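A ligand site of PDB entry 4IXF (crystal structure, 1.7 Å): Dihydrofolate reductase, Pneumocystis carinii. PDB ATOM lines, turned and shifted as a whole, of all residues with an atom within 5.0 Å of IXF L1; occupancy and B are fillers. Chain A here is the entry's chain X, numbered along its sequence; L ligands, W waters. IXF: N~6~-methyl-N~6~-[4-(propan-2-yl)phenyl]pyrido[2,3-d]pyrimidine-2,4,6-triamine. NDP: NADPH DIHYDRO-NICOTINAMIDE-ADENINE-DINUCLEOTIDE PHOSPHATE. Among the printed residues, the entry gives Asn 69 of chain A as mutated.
Water W2 lies within hydrogen-bond range of the side-chain carboxylate (OE1) of Glu 32 (2.8 Å) and a nitrogen (NAL) of IXF L1 (3.2 Å).
Water W1 lies within hydrogen-bond range of the side-chain hydroxyl of Thr 144, the backbone carbonyl oxygen of Val 11 and a nitrogen (NAD) of IXF L1.
Merely in contact with IXF L1: Ala 12 (3.6 Å), Leu 25 (3.5 Å), Ile 33 (3.4 Å), Phe 36 (3.4 Å), Thr 61 (3.8 Å), Asn 69 (3.6 Å), Leu 72 (3.7 Å) and Thr 144 (3.7 Å).
Within 4 Å of IXF L1: Ile 10, Val 11, Ala 12, Leu 25, Glu 32, Ile 33, Phe 36, Thr 61, Asn 69, Leu 72, Ile 123, Tyr 129 and Thr 144.
The side-chain carboxylate of Glu 32 is in hydrogen-bond range of the side-chain hydroxyl of Thr 144.
O of Ile 10 sits at hydrogen-bond distance from OH of Tyr 129.
OH of Tyr 129 is in hydrogen-bond range of O of Ile 123, 3.3 Å away.
The backbone NH (N) of Thr 144 sits at hydrogen-bond distance from the backbone carbonyl oxygen (O) of Val 11 (2.9 Å).
The side-chain hydroxyl (OG) of Ser 64 sits at hydrogen-bond distance from the backbone carbonyl oxygen (O) of Thr 61, 2.8 Å away.
NAD of IXF L1 is in hydrogen-bond range of OE2 of Glu 32.
A nitrogen (NAE) of IXF L1 sits at hydrogen-bond distance from the backbone carbonyl oxygen (O) of Ile 10 (2.8 Å).
NAE of IXF L1 sits at hydrogen-bond distance from O of Ile 123, at 2.9 Å.
A nitrogen (NAE) of IXF L1 sits at hydrogen-bond distance from the side-chain hydroxyl of Tyr 129.
N1 of IXF L1 lies within hydrogen-bond range of N of Val 11 (3.4 Å).
The backbone carbonyl oxygen (O) of Ala 12 lies close to a nitrogen (N7N) of NDP L2, 3.4 Å away.
The backbone NH (N) of Thr 61 is in hydrogen-bond range of an oxygen (O2A) of NDP L2 (2.9 Å).
An oxygen (O2A) of NDP L2 sits at hydrogen-bond distance from the side-chain hydroxyl (OG1) of Thr 61 (2.7 Å).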
ATOM      1  N   ILE A  10       1.742   8.660 -13.836  1.00  0.00           N
ATOM      2  CA  ILE A  10       2.866   8.919 -14.778  1.00  0.00           C
ATOM      3  C   ILE A  10       4.164   8.700 -13.982  1.00  0.00           C
ATOM      4  O   ILE A  10       4.290   9.118 -12.801  1.00  0.00           O
ATOM      5  CB  ILE A  10       2.806  10.344 -15.397  1.00  0.00           C
ATOM      6  CG1 ILE A  10       4.043  10.614 -16.356  1.00  0.00           C
ATOM      7  CG2 ILE A  10       2.705  11.476 -14.330  1.00  0.00           C
ATOM      8  CD1 ILE A  10       3.743  11.660 -17.410  1.00  0.00           C
ATOM      9  N   VAL A  11       5.089   8.046 -14.642  1.00  0.00           N
ATOM     10  CA  VAL A  11       6.331   7.553 -13.987  1.00  0.00           C
ATOM     11  C   VAL A  11       7.427   7.384 -15.008  1.00  0.00           C
ATOM     12  O   VAL A  11       7.142   6.971 -16.119  1.00  0.00           O
ATOM     13  CB  VAL A  11       6.025   6.183 -13.219  1.00  0.00           C
ATOM     14  CG1 VAL A  11       5.626   5.018 -14.161  1.00  0.00           C
ATOM     15  CG2 VAL A  11       7.213   5.764 -12.312  1.00  0.00           C
ATOM     16  N   ALA A  12       8.676   7.526 -14.563  1.00  0.00           N
ATOM     17  CA  ALA A  12       9.839   7.185 -15.345  1.00  0.00           C
ATOM     18  C   ALA A  12      10.549   6.147 -14.493  1.00  0.00           C
ATOM     19  O   ALA A  12      10.715   6.322 -13.226  1.00  0.00           O
ATOM     20  CB  ALA A  12      10.726   8.406 -15.556  1.00  0.00           C
ATOM     21  N   LEU A  25      15.899  12.019  -8.411  1.00  0.00           N
ATOM     22  CA  LEU A  25      15.856  11.144  -9.593  1.00  0.00           C
ATOM     23  C   LEU A  25      17.260  10.767  -9.935  1.00  0.00           C
ATOM     24  O   LEU A  25      18.131  11.646  -9.932  1.00  0.00           O
ATOM     25  CB  LEU A  25      15.245  11.932 -10.778  1.00  0.00           C
ATOM     26  CG  LEU A  25      13.865  12.507 -10.539  1.00  0.00           C
ATOM     27  CD1 LEU A  25      13.472  13.387 -11.705  1.00  0.00           C
ATOM     28  CD2 LEU A  25      12.918  11.310 -10.373  1.00  0.00           C
ATOM     29  N   GLU A  32      13.015  14.321 -21.051  1.00  0.00           N
ATOM     30  CA  GLU A  32      12.076  13.461 -20.280  1.00  0.00           C
ATOM     31  C   GLU A  32      11.262  14.389 -19.353  1.00  0.00           C
ATOM     32  O   GLU A  32      10.020  14.309 -19.329  1.00  0.00           O
ATOM     33  CB  GLU A  32      12.771  12.342 -19.498  1.00  0.00           C
ATOM     34  CG  GLU A  32      11.856  11.107 -19.253  1.00  0.00           C
ATOM     35  CD  GLU A  32      10.692  11.333 -18.293  1.00  0.00           C
ATOM     36  OE1 GLU A  32      10.881  11.914 -17.190  1.00  0.00           O
ATOM     37  OE2 GLU A  32       9.572  10.919 -18.615  1.00  0.00           O
ATOM     38  N   ILE A  33      11.903  15.289 -18.641  1.00  0.00           N
ATOM     39  CA  ILE A  33      11.167  16.258 -17.802  1.00  0.00           C
ATOM     40  C   ILE A  33      10.205  17.095 -18.662  1.00  0.00           C
ATOM     41  O   ILE A  33       9.085  17.428 -18.232  1.00  0.00           O
ATOM     42  CB  ILE A  33      12.171  17.157 -17.030  1.00  0.00           C
ATOM     43  CG1 ILE A  33      12.923  16.308 -16.006  1.00  0.00           C
ATOM     44  CG2 ILE A  33      11.494  18.406 -16.417  1.00  0.00           C
ATOM     45  CD1 ILE A  33      12.234  16.174 -14.664  1.00  0.00           C
ATOM     46  N   TYR A  35       8.688  16.171 -21.538  1.00  0.00           N
ATOM     47  CA  TYR A  35       7.558  15.244 -21.765  1.00  0.00           C
ATOM     48  C   TYR A  35       6.626  15.228 -20.524  1.00  0.00           C
ATOM     49  O   TYR A  35       5.425  15.371 -20.659  1.00  0.00           O
ATOM     50  CB  TYR A  35       8.087  13.832 -21.972  1.00  0.00           C
ATOM     51  CG  TYR A  35       6.988  12.817 -22.185  1.00  0.00           C
ATOM     52  CD1 TYR A  35       6.279  12.743 -23.417  1.00  0.00           C
ATOM     53  CD2 TYR A  35       6.649  11.901 -21.180  1.00  0.00           C
ATOM     54  CE1 TYR A  35       5.319  11.778 -23.641  1.00  0.00           C
ATOM     55  CE2 TYR A  35       5.691  10.943 -21.410  1.00  0.00           C
ATOM     56  CZ  TYR A  35       5.026  10.881 -22.641  1.00  0.00           C
ATOM     57  OH  TYR A  35       4.033   9.928 -22.852  1.00  0.00           O
ATOM     58  N   PHE A  36       7.195  15.024 -19.328  1.00  0.00           N
ATOM     59  CA  PHE A  36       6.406  15.069 -18.070  1.00  0.00           C
ATOM     60  C   PHE A  36       5.591  16.345 -17.952  1.00  0.00           C
ATOM     61  O   PHE A  36       4.373  16.291 -17.676  1.00  0.00           O
ATOM     62  CB  PHE A  36       7.301  14.880 -16.814  1.00  0.00           C
ATOM     63  CG  PHE A  36       6.608  15.172 -15.496  1.00  0.00           C
ATOM     64  CD1 PHE A  36       5.791  14.191 -14.836  1.00  0.00           C
ATOM     65  CD2 PHE A  36       6.765  16.420 -14.907  1.00  0.00           C
ATOM     66  CE1 PHE A  36       5.153  14.561 -13.637  1.00  0.00           C
ATOM     67  CE2 PHE A  36       6.154  16.764 -13.707  1.00  0.00           C
ATOM     68  CZ  PHE A  36       5.350  15.812 -13.057  1.00  0.00           C
ATOM     69  N   THR A  61       8.049  13.153  -2.361  1.00  0.00           N
ATOM     70  CA  THR A  61       8.123  13.733  -3.712  1.00  0.00           C
ATOM     71  C   THR A  61       7.995  15.234  -3.676  1.00  0.00           C
ATOM     72  O   THR A  61       8.734  15.939  -4.417  1.00  0.00           O
ATOM     73  CB  THR A  61       7.097  13.090  -4.666  1.00  0.00           C
ATOM     74  OG1 THR A  61       7.428  11.714  -4.746  1.00  0.00           O
ATOM     75  CG2 THR A  61       7.140  13.724  -6.080  1.00  0.00           C
ATOM     76  N   SER A  64      11.258  16.592  -2.740  1.00  0.00           N
ATOM     77  CA  SER A  64      12.261  16.339  -3.778  1.00  0.00           C
ATOM     78  C   SER A  64      12.241  17.374  -4.888  1.00  0.00           C
ATOM     79  O   SER A  64      13.214  17.441  -5.672  1.00  0.00           O
ATOM     80  CB  SER A  64      12.083  14.939  -4.364  1.00  0.00           C
ATOM     81  OG  SER A  64      11.106  14.969  -5.430  1.00  0.00           O
ATOM     82  N   ILE A  65      11.177  18.189  -4.984  1.00  0.00           N
ATOM     83  CA  ILE A  65      11.113  19.175  -6.043  1.00  0.00           C
ATOM     84  C   ILE A  65      11.927  20.408  -5.591  1.00  0.00           C
ATOM     85  O   ILE A  65      11.756  20.838  -4.447  1.00  0.00           O
ATOM     86  CB  ILE A  65       9.654  19.601  -6.387  1.00  0.00           C
ATOM     87  CG1 ILE A  65       8.859  18.396  -6.920  1.00  0.00           C
ATOM     88  CG2 ILE A  65       9.645  20.709  -7.436  1.00  0.00           C
ATOM     89  CD1 ILE A  65       7.360  18.498  -6.753  1.00  0.00           C
ATOM     90  N   PRO A  66      12.835  20.944  -6.470  1.00  0.00           N
ATOM     91  CA  PRO A  66      13.575  22.096  -5.967  1.00  0.00           C
ATOM     92  C   PRO A  66      12.615  23.131  -5.445  1.00  0.00           C
ATOM     93  O   PRO A  66      11.585  23.371  -6.084  1.00  0.00           O
ATOM     94  CB  PRO A  66      14.345  22.580  -7.214  1.00  0.00           C
ATOM     95  CG  PRO A  66      14.643  21.321  -7.977  1.00  0.00           C
ATOM     96  CD  PRO A  66      13.405  20.423  -7.727  1.00  0.00           C
ATOM     97  N   ASN A  69      10.986  25.544  -7.678  1.00  0.00           N
ATOM     98  CA  ASN A  69      10.124  24.926  -8.700  1.00  0.00           C
ATOM     99  C   ASN A  69       8.739  24.454  -8.230  1.00  0.00           C
ATOM    100  O   ASN A  69       7.965  23.899  -9.040  1.00  0.00           O
ATOM    101  CB  ASN A  69      10.869  23.758  -9.294  1.00  0.00           C
ATOM    102  CG  ASN A  69      11.995  24.208 -10.138  1.00  0.00           C
ATOM    103  OD1 ASN A  69      11.791  24.978 -11.072  1.00  0.00           O
ATOM    104  ND2 ASN A  69      13.212  23.743  -9.829  1.00  0.00           N
ATOM    105  N   LEU A  72       4.301  22.850  -8.681  1.00  0.00           N
ATOM    106  CA  LEU A  72       4.555  22.654 -10.101  1.00  0.00           C
ATOM    107  C   LEU A  72       3.614  23.535 -10.909  1.00  0.00           C
ATOM    108  O   LEU A  72       2.361  23.445 -10.783  1.00  0.00           O
ATOM    109  CB  LEU A  72       4.388  21.165 -10.477  1.00  0.00           C
ATOM    110  CG  LEU A  72       5.513  20.243 -10.010  1.00  0.00           C
ATOM    111  CD1 LEU A  72       5.111  18.819 -10.407  1.00  0.00           C
ATOM    112  CD2 LEU A  72       6.860  20.641 -10.655  1.00  0.00           C
ATOM    113  N   ILE A 123       1.748  11.443  -9.547  1.00  0.00           N
ATOM    114  CA  ILE A 123       3.105  11.686 -10.121  1.00  0.00           C
ATOM    115  C   ILE A 123       4.217  11.114  -9.219  1.00  0.00           C
ATOM    116  O   ILE A 123       5.418  11.356  -9.465  1.00  0.00           O
ATOM    117  CB  ILE A 123       3.386  13.186 -10.426  1.00  0.00           C
ATOM    118  CG1 ILE A 123       3.438  14.004  -9.120  1.00  0.00           C
ATOM    119  CG2 ILE A 123       2.328  13.741 -11.394  1.00  0.00           C
ATOM    120  CD1 ILE A 123       4.186  15.343  -9.231  1.00  0.00           C
ATOM    121  N   GLY A 124       3.821  10.298  -8.227  1.00  0.00           N
ATOM    122  CA  GLY A 124       4.785   9.638  -7.325  1.00  0.00           C
ATOM    123  C   GLY A 124       4.682  10.067  -5.837  1.00  0.00           C
ATOM    124  O   GLY A 124       3.859  10.931  -5.497  1.00  0.00           O
ATOM    125  N   TYR A 129       2.242   5.687  -5.299  1.00  0.00           N
ATOM    126  CA  TYR A 129       1.990   4.916  -6.495  1.00  0.00           C
ATOM    127  C   TYR A 129       1.368   3.582  -6.039  1.00  0.00           C
ATOM    128  O   TYR A 129       0.534   3.009  -6.702  1.00  0.00           O
ATOM    129  CB  TYR A 129       3.255   4.522  -7.215  1.00  0.00           C
ATOM    130  CG  TYR A 129       3.864   5.587  -8.126  1.00  0.00           C
ATOM    131  CD1 TYR A 129       3.044   6.443  -8.894  1.00  0.00           C
ATOM    132  CD2 TYR A 129       5.231   5.655  -8.240  1.00  0.00           C
ATOM    133  CE1 TYR A 129       3.684   7.385  -9.780  1.00  0.00           C
ATOM    134  CE2 TYR A 129       5.848   6.562  -9.097  1.00  0.00           C
ATOM    135  CZ  TYR A 129       5.032   7.459  -9.824  1.00  0.00           C
ATOM    136  OH  TYR A 129       5.748   8.344 -10.663  1.00  0.00           O
ATOM    137  N   THR A 144       7.782   5.996 -18.742  1.00  0.00           N
ATOM    138  CA  THR A 144       9.006   6.175 -19.548  1.00  0.00           C
ATOM    139  C   THR A 144       9.933   5.054 -19.122  1.00  0.00           C
ATOM    140  O   THR A 144      10.309   5.026 -17.951  1.00  0.00           O
ATOM    141  CB  THR A 144       9.651   7.509 -19.299  1.00  0.00           C
ATOM    142  OG1 THR A 144       8.696   8.510 -19.620  1.00  0.00           O
ATOM    143  CG2 THR A 144      10.915   7.645 -20.202  1.00  0.00           C
HETATM  144  CAA IXF L   1      10.298  21.258 -11.858  1.00  0.00           C
HETATM  145  CAV IXF L   1      11.455  20.246 -11.639  1.00  0.00           C
HETATM  146  CAB IXF L   1      12.433  20.223 -12.826  1.00  0.00           C
HETATM  147  CAQ IXF L   1      10.910  18.799 -11.361  1.00  0.00           C
HETATM  148  CAG IXF L   1      11.538  18.007 -10.405  1.00  0.00           C
HETATM  149  CAI IXF L   1      11.070  16.699 -10.122  1.00  0.00           C
HETATM  150  CAF IXF L   1       9.816  18.251 -12.048  1.00  0.00           C
HETATM  151  CAH IXF L   1       9.375  16.968 -11.758  1.00  0.00           C
HETATM  152  CAR IXF L   1       9.992  16.152 -10.816  1.00  0.00           C
HETATM  153  NAW IXF L   1       9.526  14.834 -10.613  1.00  0.00           N
HETATM  154  CAC IXF L   1       8.938  14.408  -9.353  1.00  0.00           C
HETATM  155  CAS IXF L   1       9.357  14.054 -11.727  1.00  0.00           C
HETATM  156  CAK IXF L   1       8.236  13.158 -11.819  1.00  0.00           C
HETATM  157  C5  IXF L   1       8.099  12.419 -12.982  1.00  0.00           C
HETATM  158  C6  IXF L   1       7.016  11.490 -13.207  1.00  0.00           C
HETATM  159  NAE IXF L   1       6.032  11.287 -12.282  1.00  0.00           N
HETATM  160  N1  IXF L   1       6.966  10.895 -14.383  1.00  0.00           N
HETATM  161  C2  IXF L   1       7.867  11.072 -15.379  1.00  0.00           C
HETATM  162  NAD IXF L   1       7.822  10.437 -16.592  1.00  0.00           N
HETATM  163  N3  IXF L   1       8.919  11.895 -15.168  1.00  0.00           N
HETATM  164  C4  IXF L   1       9.041  12.602 -14.029  1.00  0.00           C
HETATM  165  NAL IXF L   1      10.127  13.457 -13.947  1.00  0.00           N
HETATM  166  CAJ IXF L   1      10.251  14.149 -12.807  1.00  0.00           C
HETATM  167  PA  NDP L   2       6.395   9.468  -1.598  1.00  0.00           P
HETATM  168  O1A NDP L   2       5.408   8.360  -1.913  1.00  0.00           O
HETATM  169  O2A NDP L   2       6.569  10.695  -2.356  1.00  0.00           O
HETATM  170  O5B NDP L   2       6.153  10.067  -0.044  1.00  0.00           O
HETATM  171  C5B NDP L   2       5.683   9.120   0.935  1.00  0.00           C
HETATM  172  C4B NDP L   2       5.024   9.936   1.992  1.00  0.00           C
HETATM  173  O4B NDP L   2       3.855  10.625   1.412  1.00  0.00           O
HETATM  174  C3B NDP L   2       4.536   9.061   3.179  1.00  0.00           C
HETATM  175  O3B NDP L   2       5.539   9.126   4.231  1.00  0.00           O
HETATM  176  C2B NDP L   2       3.309   9.851   3.571  1.00  0.00           C
HETATM  177  O2B NDP L   2       3.593  11.110   4.079  1.00  0.00           O
HETATM  178  C1B NDP L   2       2.690  10.214   2.190  1.00  0.00           C
HETATM  179  N9A NDP L   2       1.896   9.174   1.543  1.00  0.00           N
HETATM  180  C8A NDP L   2       2.216   8.431   0.462  1.00  0.00           C
HETATM  181  N7A NDP L   2       1.245   7.585   0.160  1.00  0.00           N
HETATM  182  C5A NDP L   2       0.230   7.853   1.033  1.00  0.00           C
HETATM  183  C6A NDP L   2      -1.053   7.344   1.220  1.00  0.00           C
HETATM  184  N6A NDP L   2      -1.580   6.390   0.430  1.00  0.00           N
HETATM  185  N1A NDP L   2      -1.783   7.847   2.235  1.00  0.00           N
HETATM  186  C2A NDP L   2      -1.340   8.804   3.066  1.00  0.00           C
HETATM  187  N3A NDP L   2      -0.123   9.319   2.930  1.00  0.00           N
HETATM  188  C4A NDP L   2       0.664   8.838   1.932  1.00  0.00           C
HETATM  189  O3  NDP L   2       7.806   8.845  -1.232  1.00  0.00           O
HETATM  190  PN  NDP L   2       8.627   7.649  -1.647  1.00  0.00           P
HETATM  191  O1N NDP L   2       7.867   6.365  -1.793  1.00  0.00           O
HETATM  192  O2N NDP L   2       9.881   7.588  -0.744  1.00  0.00           O
HETATM  193  O5D NDP L   2       9.206   7.989  -3.024  1.00  0.00           O
HETATM  194  C5D NDP L   2       9.947   9.267  -3.284  1.00  0.00           C
HETATM  195  C4D NDP L   2      11.163   8.928  -4.158  1.00  0.00           C
HETATM  196  O4D NDP L   2      10.495   8.689  -5.430  1.00  0.00           O
HETATM  197  C3D NDP L   2      12.208  10.022  -4.442  1.00  0.00           C
HETATM  198  O3D NDP L   2      13.440   9.398  -4.832  1.00  0.00           O
HETATM  199  C2D NDP L   2      11.674  10.691  -5.681  1.00  0.00           C
HETATM  200  O2D NDP L   2      12.728  11.306  -6.453  1.00  0.00           O
HETATM  201  C1D NDP L   2      11.154   9.508  -6.472  1.00  0.00           C
HETATM  202  N1N NDP L   2      10.154   9.835  -7.550  1.00  0.00           N
HETATM  203  C2N NDP L   2      10.437   9.279  -8.827  1.00  0.00           C
HETATM  204  C3N NDP L   2       9.546   9.465  -9.867  1.00  0.00           C
HETATM  205  C7N NDP L   2       9.914   8.917 -11.291  1.00  0.00           C
HETATM  206  O7N NDP L   2      11.043   8.407 -11.583  1.00  0.00           O
HETATM  207  N7N NDP L   2       8.901   9.028 -12.120  1.00  0.00           N
HETATM  208  C4N NDP L   2       8.422  10.304  -9.647  1.00  0.00           C
HETATM  209  C5N NDP L   2       8.148  10.810  -8.370  1.00  0.00           C
HETATM  210  C6N NDP L   2       9.018  10.575  -7.299  1.00  0.00           C
HETATM  211  P2B NDP L   2       3.795  11.500   5.742  1.00  0.00           P
HETATM  212  O1X NDP L   2       5.060  10.709   6.088  1.00  0.00           O
HETATM  213  O2X NDP L   2       3.899  12.988   5.744  1.00  0.00           O
HETATM  214  O3X NDP L   2       2.513  10.809   6.506  1.00  0.00           O
HETATM  215  O   HOH W   1       5.954   8.604 -18.766  1.00  0.00           O
HETATM  216  O   HOH W   2      12.766  12.194 -15.206  1.00  0.00           O
